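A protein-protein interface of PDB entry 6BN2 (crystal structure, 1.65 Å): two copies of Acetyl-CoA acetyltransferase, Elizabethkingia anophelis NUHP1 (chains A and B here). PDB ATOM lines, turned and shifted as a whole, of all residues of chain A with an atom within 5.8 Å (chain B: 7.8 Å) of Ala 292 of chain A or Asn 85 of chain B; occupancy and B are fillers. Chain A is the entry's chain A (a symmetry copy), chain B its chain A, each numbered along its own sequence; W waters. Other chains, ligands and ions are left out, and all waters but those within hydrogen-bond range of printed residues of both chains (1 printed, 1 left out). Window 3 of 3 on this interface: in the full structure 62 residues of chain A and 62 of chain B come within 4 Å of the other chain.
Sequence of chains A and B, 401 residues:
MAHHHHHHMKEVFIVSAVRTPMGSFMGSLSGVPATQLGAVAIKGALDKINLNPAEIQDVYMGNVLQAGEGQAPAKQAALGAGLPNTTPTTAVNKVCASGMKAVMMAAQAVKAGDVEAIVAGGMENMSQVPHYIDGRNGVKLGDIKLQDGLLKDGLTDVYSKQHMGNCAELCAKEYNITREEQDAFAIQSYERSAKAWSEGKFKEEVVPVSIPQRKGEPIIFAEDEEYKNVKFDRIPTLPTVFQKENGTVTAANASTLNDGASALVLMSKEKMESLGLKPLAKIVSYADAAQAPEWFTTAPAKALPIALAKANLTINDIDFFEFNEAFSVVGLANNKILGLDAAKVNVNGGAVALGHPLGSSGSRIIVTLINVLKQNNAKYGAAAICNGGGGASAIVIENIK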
ATOM      1  N   ALA A 290     -14.951  -6.064  -4.857  1.00  0.00           N
ATOM      2  CA  ALA A 290     -15.608  -5.730  -3.600  1.00  0.00           C
ATOM      3  C   ALA A 290     -15.654  -6.944  -2.691  1.00  0.00           C
ATOM      4  O   ALA A 290     -15.646  -8.089  -3.149  1.00  0.00           O
ATOM      5  CB  ALA A 290     -17.031  -5.189  -3.849  1.00  0.00           C
ATOM      6  N   GLN A 291     -15.714  -6.685  -1.390  1.00  0.00           N
ATOM      7  CA  GLN A 291     -15.989  -7.738  -0.422  1.00  0.00           C
ATOM      8  C   GLN A 291     -16.857  -7.135   0.681  1.00  0.00           C
ATOM      9  O   GLN A 291     -17.482  -6.080   0.504  1.00  0.00           O
ATOM     10  CB  GLN A 291     -14.674  -8.367   0.069  1.00  0.00           C
ATOM     11  CG  GLN A 291     -13.628  -7.351   0.314  1.00  0.00           C
ATOM     12  CD  GLN A 291     -12.208  -7.910   0.505  1.00  0.00           C
ATOM     13  OE1 GLN A 291     -11.788  -8.906  -0.099  1.00  0.00           O
ATOM     14  NE2 GLN A 291     -11.467  -7.248   1.348  1.00  0.00           N
ATOM     15  N   ALA A 292     -16.944  -7.829   1.816  1.00  0.00           N
ATOM     16  CA  ALA A 292     -17.819  -7.364   2.887  1.00  0.00           C
ATOM     17  C   ALA A 292     -17.503  -5.909   3.228  1.00  0.00           C
ATOM     18  O   ALA A 292     -16.329  -5.519   3.218  1.00  0.00           O
ATOM     19  CB  ALA A 292     -17.649  -8.231   4.135  1.00  0.00           C
ATOM     20  N   PRO A 293     -18.513  -5.081   3.512  1.00  0.00           N
ATOM     21  CA  PRO A 293     -18.250  -3.660   3.793  1.00  0.00           C
ATOM     22  C   PRO A 293     -17.198  -3.432   4.862  1.00  0.00           C
ATOM     23  O   PRO A 293     -16.368  -2.525   4.711  1.00  0.00           O
ATOM     24  CB  PRO A 293     -19.628  -3.140   4.235  1.00  0.00           C
ATOM     25  CG  PRO A 293     -20.600  -3.977   3.389  1.00  0.00           C
ATOM     26  CD  PRO A 293     -19.948  -5.355   3.283  1.00  0.00           C
ATOM     27  N   GLU A 294     -17.203  -4.239   5.928  1.00  0.00           N
ATOM     28  CA  GLU A 294     -16.223  -4.055   6.987  1.00  0.00           C
ATOM     29  C   GLU A 294     -14.820  -4.434   6.539  1.00  0.00           C
ATOM     30  O   GLU A 294     -13.856  -4.125   7.253  1.00  0.00           O
ATOM     31  CB  GLU A 294     -16.620  -4.862   8.226  1.00  0.00           C
ATOM     32  CG  GLU A 294     -16.564  -6.369   8.037  1.00  0.00           C
ATOM     33  CD  GLU A 294     -17.889  -6.984   7.592  1.00  0.00           C
ATOM     34  OE1 GLU A 294     -18.703  -6.324   6.891  1.00  0.00           O
ATOM     35  OE2 GLU A 294     -18.115  -8.160   7.954  1.00  0.00           O
ATOM     36  N   TRP A 295     -14.670  -5.065   5.373  1.00  0.00           N
ATOM     37  CA  TRP A 295     -13.345  -5.399   4.857  1.00  0.00           C
ATOM     38  C   TRP A 295     -12.954  -4.557   3.649  1.00  0.00           C
ATOM     39  O   TRP A 295     -12.178  -4.999   2.800  1.00  0.00           O
ATOM     40  CB  TRP A 295     -13.266  -6.893   4.542  1.00  0.00           C
ATOM     41  CG  TRP A 295     -13.157  -7.642   5.829  1.00  0.00           C
ATOM     42  CD1 TRP A 295     -14.114  -8.425   6.425  1.00  0.00           C
ATOM     43  CD2 TRP A 295     -12.057  -7.583   6.743  1.00  0.00           C
ATOM     44  NE1 TRP A 295     -13.645  -8.890   7.637  1.00  0.00           N
ATOM     45  CE2 TRP A 295     -12.388  -8.383   7.850  1.00  0.00           C
ATOM     46  CE3 TRP A 295     -10.809  -6.944   6.714  1.00  0.00           C
ATOM     47  CZ2 TRP A 295     -11.518  -8.562   8.926  1.00  0.00           C
ATOM     48  CZ3 TRP A 295      -9.951  -7.119   7.777  1.00  0.00           C
ATOM     49  CH2 TRP A 295     -10.310  -7.921   8.868  1.00  0.00           C
ATOM     50  N   PHE A 296     -13.480  -3.329   3.551  1.00  0.00           N
ATOM     51  CA  PHE A 296     -13.022  -2.447   2.485  1.00  0.00           C
ATOM     52  C   PHE A 296     -11.512  -2.240   2.567  1.00  0.00           C
ATOM     53  O   PHE A 296     -10.859  -2.016   1.545  1.00  0.00           O
ATOM     54  CB  PHE A 296     -13.751  -1.092   2.546  1.00  0.00           C
ATOM     55  CG  PHE A 296     -13.256  -0.167   3.647  1.00  0.00           C
ATOM     56  CD1 PHE A 296     -12.139   0.642   3.455  1.00  0.00           C
ATOM     57  CD2 PHE A 296     -13.932  -0.096   4.853  1.00  0.00           C
ATOM     58  CE1 PHE A 296     -11.680   1.472   4.466  1.00  0.00           C
ATOM     59  CE2 PHE A 296     -13.487   0.737   5.859  1.00  0.00           C
ATOM     60  CZ  PHE A 296     -12.358   1.520   5.668  1.00  0.00           C
ATOM     61  N   GLY A 389     -18.242   0.733   1.779  1.00  0.00           N
ATOM     62  CA  GLY A 389     -19.140  -0.256   1.226  1.00  0.00           C
ATOM     63  C   GLY A 389     -18.450  -1.548   0.855  1.00  0.00           C
ATOM     64  O   GLY A 389     -19.137  -2.519   0.497  1.00  0.00           O
ATOM     65  N   GLY A 390     -17.120  -1.586   0.935  1.00  0.00           N
ATOM     66  CA  GLY A 390     -16.353  -2.804   0.745  1.00  0.00           C
ATOM     67  C   GLY A 390     -15.584  -2.891  -0.559  1.00  0.00           C
ATOM     68  O   GLY A 390     -15.061  -3.968  -0.880  1.00  0.00           O
ATOM     69  N   LYS B  75     -24.142   1.283  -3.397  1.00  0.00           N
ATOM     70  CA  LYS B  75     -23.941   0.018  -2.690  1.00  0.00           C
ATOM     71  C   LYS B  75     -25.163  -0.338  -1.859  1.00  0.00           C
ATOM     72  O   LYS B  75     -25.566  -1.507  -1.787  1.00  0.00           O
ATOM     73  CB  LYS B  75     -22.723   0.110  -1.774  1.00  0.00           C
ATOM     74  CG  LYS B  75     -22.414  -1.198  -1.012  1.00  0.00           C
ATOM     75  CD  LYS B  75     -21.901  -2.299  -1.912  1.00  0.00           C
ATOM     76  CE  LYS B  75     -20.590  -1.874  -2.583  1.00  0.00           C
ATOM     77  NZ  LYS B  75     -19.872  -3.022  -3.216  1.00  0.00           N
ATOM     78  N   ALA B  78     -27.697  -1.826  -4.128  1.00  0.00           N
ATOM     79  CA  ALA B  78     -27.320  -3.152  -4.616  1.00  0.00           C
ATOM     80  C   ALA B  78     -27.452  -4.208  -3.526  1.00  0.00           C
ATOM     81  O   ALA B  78     -28.020  -5.279  -3.758  1.00  0.00           O
ATOM     82  CB  ALA B  78     -25.883  -3.131  -5.157  1.00  0.00           C
ATOM     83  N   LEU B  79     -26.888  -3.947  -2.338  1.00  0.00           N
ATOM     84  CA  LEU B  79     -26.976  -4.932  -1.265  1.00  0.00           C
ATOM     85  C   LEU B  79     -28.424  -5.133  -0.824  1.00  0.00           C
ATOM     86  O   LEU B  79     -28.842  -6.263  -0.528  1.00  0.00           O
ATOM     87  CB  LEU B  79     -26.099  -4.515  -0.079  1.00  0.00           C
ATOM     88  CG  LEU B  79     -24.603  -4.474  -0.373  1.00  0.00           C
ATOM     89  CD1 LEU B  79     -23.836  -4.033   0.880  1.00  0.00           C
ATOM     90  CD2 LEU B  79     -24.094  -5.838  -0.862  1.00  0.00           C
ATOM     91  N   GLY B  82     -30.260  -7.687  -2.811  1.00  0.00           N
ATOM     92  CA  GLY B  82     -29.782  -9.044  -2.725  1.00  0.00           C
ATOM     93  C   GLY B  82     -28.570  -9.357  -3.569  1.00  0.00           C
ATOM     94  O   GLY B  82     -28.209 -10.537  -3.681  1.00  0.00           O
ATOM     95  N   LEU B  83     -27.956  -8.353  -4.198  1.00  0.00           N
ATOM     96  CA  LEU B  83     -26.679  -8.595  -4.857  1.00  0.00           C
ATOM     97  C   LEU B  83     -25.619  -8.870  -3.796  1.00  0.00           C
ATOM     98  O   LEU B  83     -25.695  -8.333  -2.685  1.00  0.00           O
ATOM     99  CB  LEU B  83     -26.271  -7.401  -5.712  1.00  0.00           C
ATOM    100  CG  LEU B  83     -27.153  -7.235  -6.964  1.00  0.00           C
ATOM    101  CD1 LEU B  83     -26.947  -5.896  -7.642  1.00  0.00           C
ATOM    102  CD2 LEU B  83     -26.827  -8.347  -7.950  1.00  0.00           C
ATOM    103  N   PRO B  84     -24.635  -9.710  -4.100  1.00  0.00           N
ATOM    104  CA  PRO B  84     -23.628 -10.055  -3.087  1.00  0.00           C
ATOM    105  C   PRO B  84     -22.659  -8.905  -2.833  1.00  0.00           C
ATOM    106  O   PRO B  84     -22.545  -7.969  -3.622  1.00  0.00           O
ATOM    107  CB  PRO B  84     -22.906 -11.260  -3.700  1.00  0.00           C
ATOM    108  CG  PRO B  84     -23.064 -11.085  -5.165  1.00  0.00           C
ATOM    109  CD  PRO B  84     -24.473 -10.507  -5.328  1.00  0.00           C
ATOM    110  N   ASN B  85     -21.940  -9.016  -1.708  1.00  0.00           N
ATOM    111  CA  ASN B  85     -20.961  -7.990  -1.343  1.00  0.00           C
ATOM    112  C   ASN B  85     -19.726  -8.022  -2.232  1.00  0.00           C
ATOM    113  O   ASN B  85     -18.807  -7.215  -2.023  1.00  0.00           O
ATOM    114  CB  ASN B  85     -20.592  -8.132   0.148  1.00  0.00           C
ATOM    115  CG  ASN B  85     -19.898  -9.451   0.492  1.00  0.00           C
ATOM    116  OD1 ASN B  85     -19.262 -10.091  -0.344  1.00  0.00           O
ATOM    117  ND2 ASN B  85     -20.003  -9.846   1.756  1.00  0.00           N
ATOM    118  N   THR B  86     -19.689  -8.917  -3.218  1.00  0.00           N
ATOM    119  CA  THR B  86     -18.638  -8.934  -4.224  1.00  0.00           C
ATOM    120  C   THR B  86     -18.982  -8.070  -5.439  1.00  0.00           C
ATOM    121  O   THR B  86     -18.209  -8.045  -6.402  1.00  0.00           O
ATOM    122  CB  THR B  86     -18.342 -10.386  -4.645  1.00  0.00           C
ATOM    123  OG1 THR B  86     -19.575 -11.039  -5.014  1.00  0.00           O
ATOM    124  CG2 THR B  86     -17.704 -11.164  -3.481  1.00  0.00           C
ATOM    125  N   THR B  87     -20.115  -7.358  -5.412  1.00  0.00           N
ATOM    126  CA  THR B  87     -20.567  -6.545  -6.541  1.00  0.00           C
ATOM    127  C   THR B  87     -20.070  -5.106  -6.430  1.00  0.00           C
ATOM    128  O   THR B  87     -20.507  -4.381  -5.522  1.00  0.00           O
ATOM    129  CB  THR B  87     -22.091  -6.527  -6.609  1.00  0.00           C
ATOM    130  OG1 THR B  87     -22.593  -7.860  -6.445  1.00  0.00           O
ATOM    131  CG2 THR B  87     -22.561  -5.968  -7.959  1.00  0.00           C
ATOM    132  N   PRO B  88     -19.236  -4.629  -7.357  1.00  0.00           N
ATOM    133  CA  PRO B  88     -18.902  -3.189  -7.382  1.00  0.00           C
ATOM    134  C   PRO B  88     -20.121  -2.326  -7.689  1.00  0.00           C
ATOM    135  O   PRO B  88     -21.036  -2.743  -8.406  1.00  0.00           O
ATOM    136  CB  PRO B  88     -17.872  -3.084  -8.515  1.00  0.00           C
ATOM    137  CG  PRO B  88     -17.270  -4.487  -8.587  1.00  0.00           C
ATOM    138  CD  PRO B  88     -18.470  -5.388  -8.357  1.00  0.00           C
HETATM  139  O   HOH W   1     -15.458  -8.421  -6.475  1.00  0.00           O
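Among the printed residues, merely in contact across the chains: Ala 290 of chain A with Thr 86 of chain B (3.3 Å), Gly 389 of chain A with Lys 75 of chain B (3.5 Å), Ala 292 of chain A with Asn 85 of chain B (3.5 Å), Ala 290 of chain A with Lys 75 of chain B (3.6 Å) and Ala 290 of chain A with Thr 87 of chain B (3.9 Å).
The backbone carbonyl oxygen of Asn 85 of chain B lies close to the backbone carbonyl oxygen of Ala 290 of chain A.
The backbone NH (N) of Gln 291 of chain A lies within hydrogen-bond range of the backbone carbonyl oxygen (O) of Asn 85 of chain B (3.2 Å).
Along chain B the printed residues that touch a printed residue of chain A span positions 75 to 87.
Printed residues of chain A that touch a printed residue of chain B: Ala 290, Gln 291, Ala 292 and Gly 389.
Hydrophobic or aromatic side chains of chain A within 4 Å of the printed part of chain B: Ala 290 and Ala 292.
Among the printed residues, 7 pairs touch across the chains.
Among the printed residues, no Asp or Glu carboxylate lies within 4 Å of a Lys or Arg side-chain nitrogen of the other chain.
Water W1 lies within hydrogen-bond range of the backbone carbonyl oxygen of Thr 86 of chain B (2.8 Å) and the backbone NH of Ala 290 of chain A (2.9 Å).
No position is printed for both chains.
Of the 7 pairs that touch across the chains among the printed residues, none has its exchanged pair printed and touching as well.
The side-chain amide nitrogen (NE2) of Gln 291 of chain A is in hydrogen-bond range of the backbone carbonyl oxygen (O) of Trp 295 of chain A (2.8 Å).
The backbone carbonyl oxygen (O) of Pro 84 of chain B is in hydrogen-bond range of the side-chain hydroxyl (OG1) of Thr 87 of chain B (2.8 Å).
The backbone carbonyl oxygen (O) of Thr 87 of chain B sits at hydrogen-bond distance from the side-chain amino group (NZ) of Lys 75 of chain B (2.8 Å).
The backbone NH (N) of Gln 291 of chain A lies within hydrogen-bond range of the backbone carbonyl oxygen (O) of Gly 390 of chain A (2.8 Å).
Ala 292 of chain A touches just one residue of chain B: Asn 85 (3.5 Å).
Of chain A, only Ala 290 (3.2 Å), Gln 291 (3.1 Å) and Ala 292 (3.5 Å) come within 4 Å of Asn 85 of chain B.
Printed residues of chain A within 4 Å of Thr 86 of chain B: Ala 290.
Of the printed residues of chain B, Ala 290 of chain A touches Lys 75, Asn 85, Thr 86 and Thr 87.
Of the printed residues of chain B, Gln 291 of chain A touches Asn 85.
Ala 78 of chain B touches none of the printed residues of chain A.
Pro 88 of chain B touches none of the printed residues of chain A.
The nearest residue of chain B that does not touch Ala 292 of chain A is Thr 86 of chain B (5.8 Å).
The nearest residue of chain A that does not touch Asn 85 of chain B is Pro 293 of chain A (4.2 Å).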
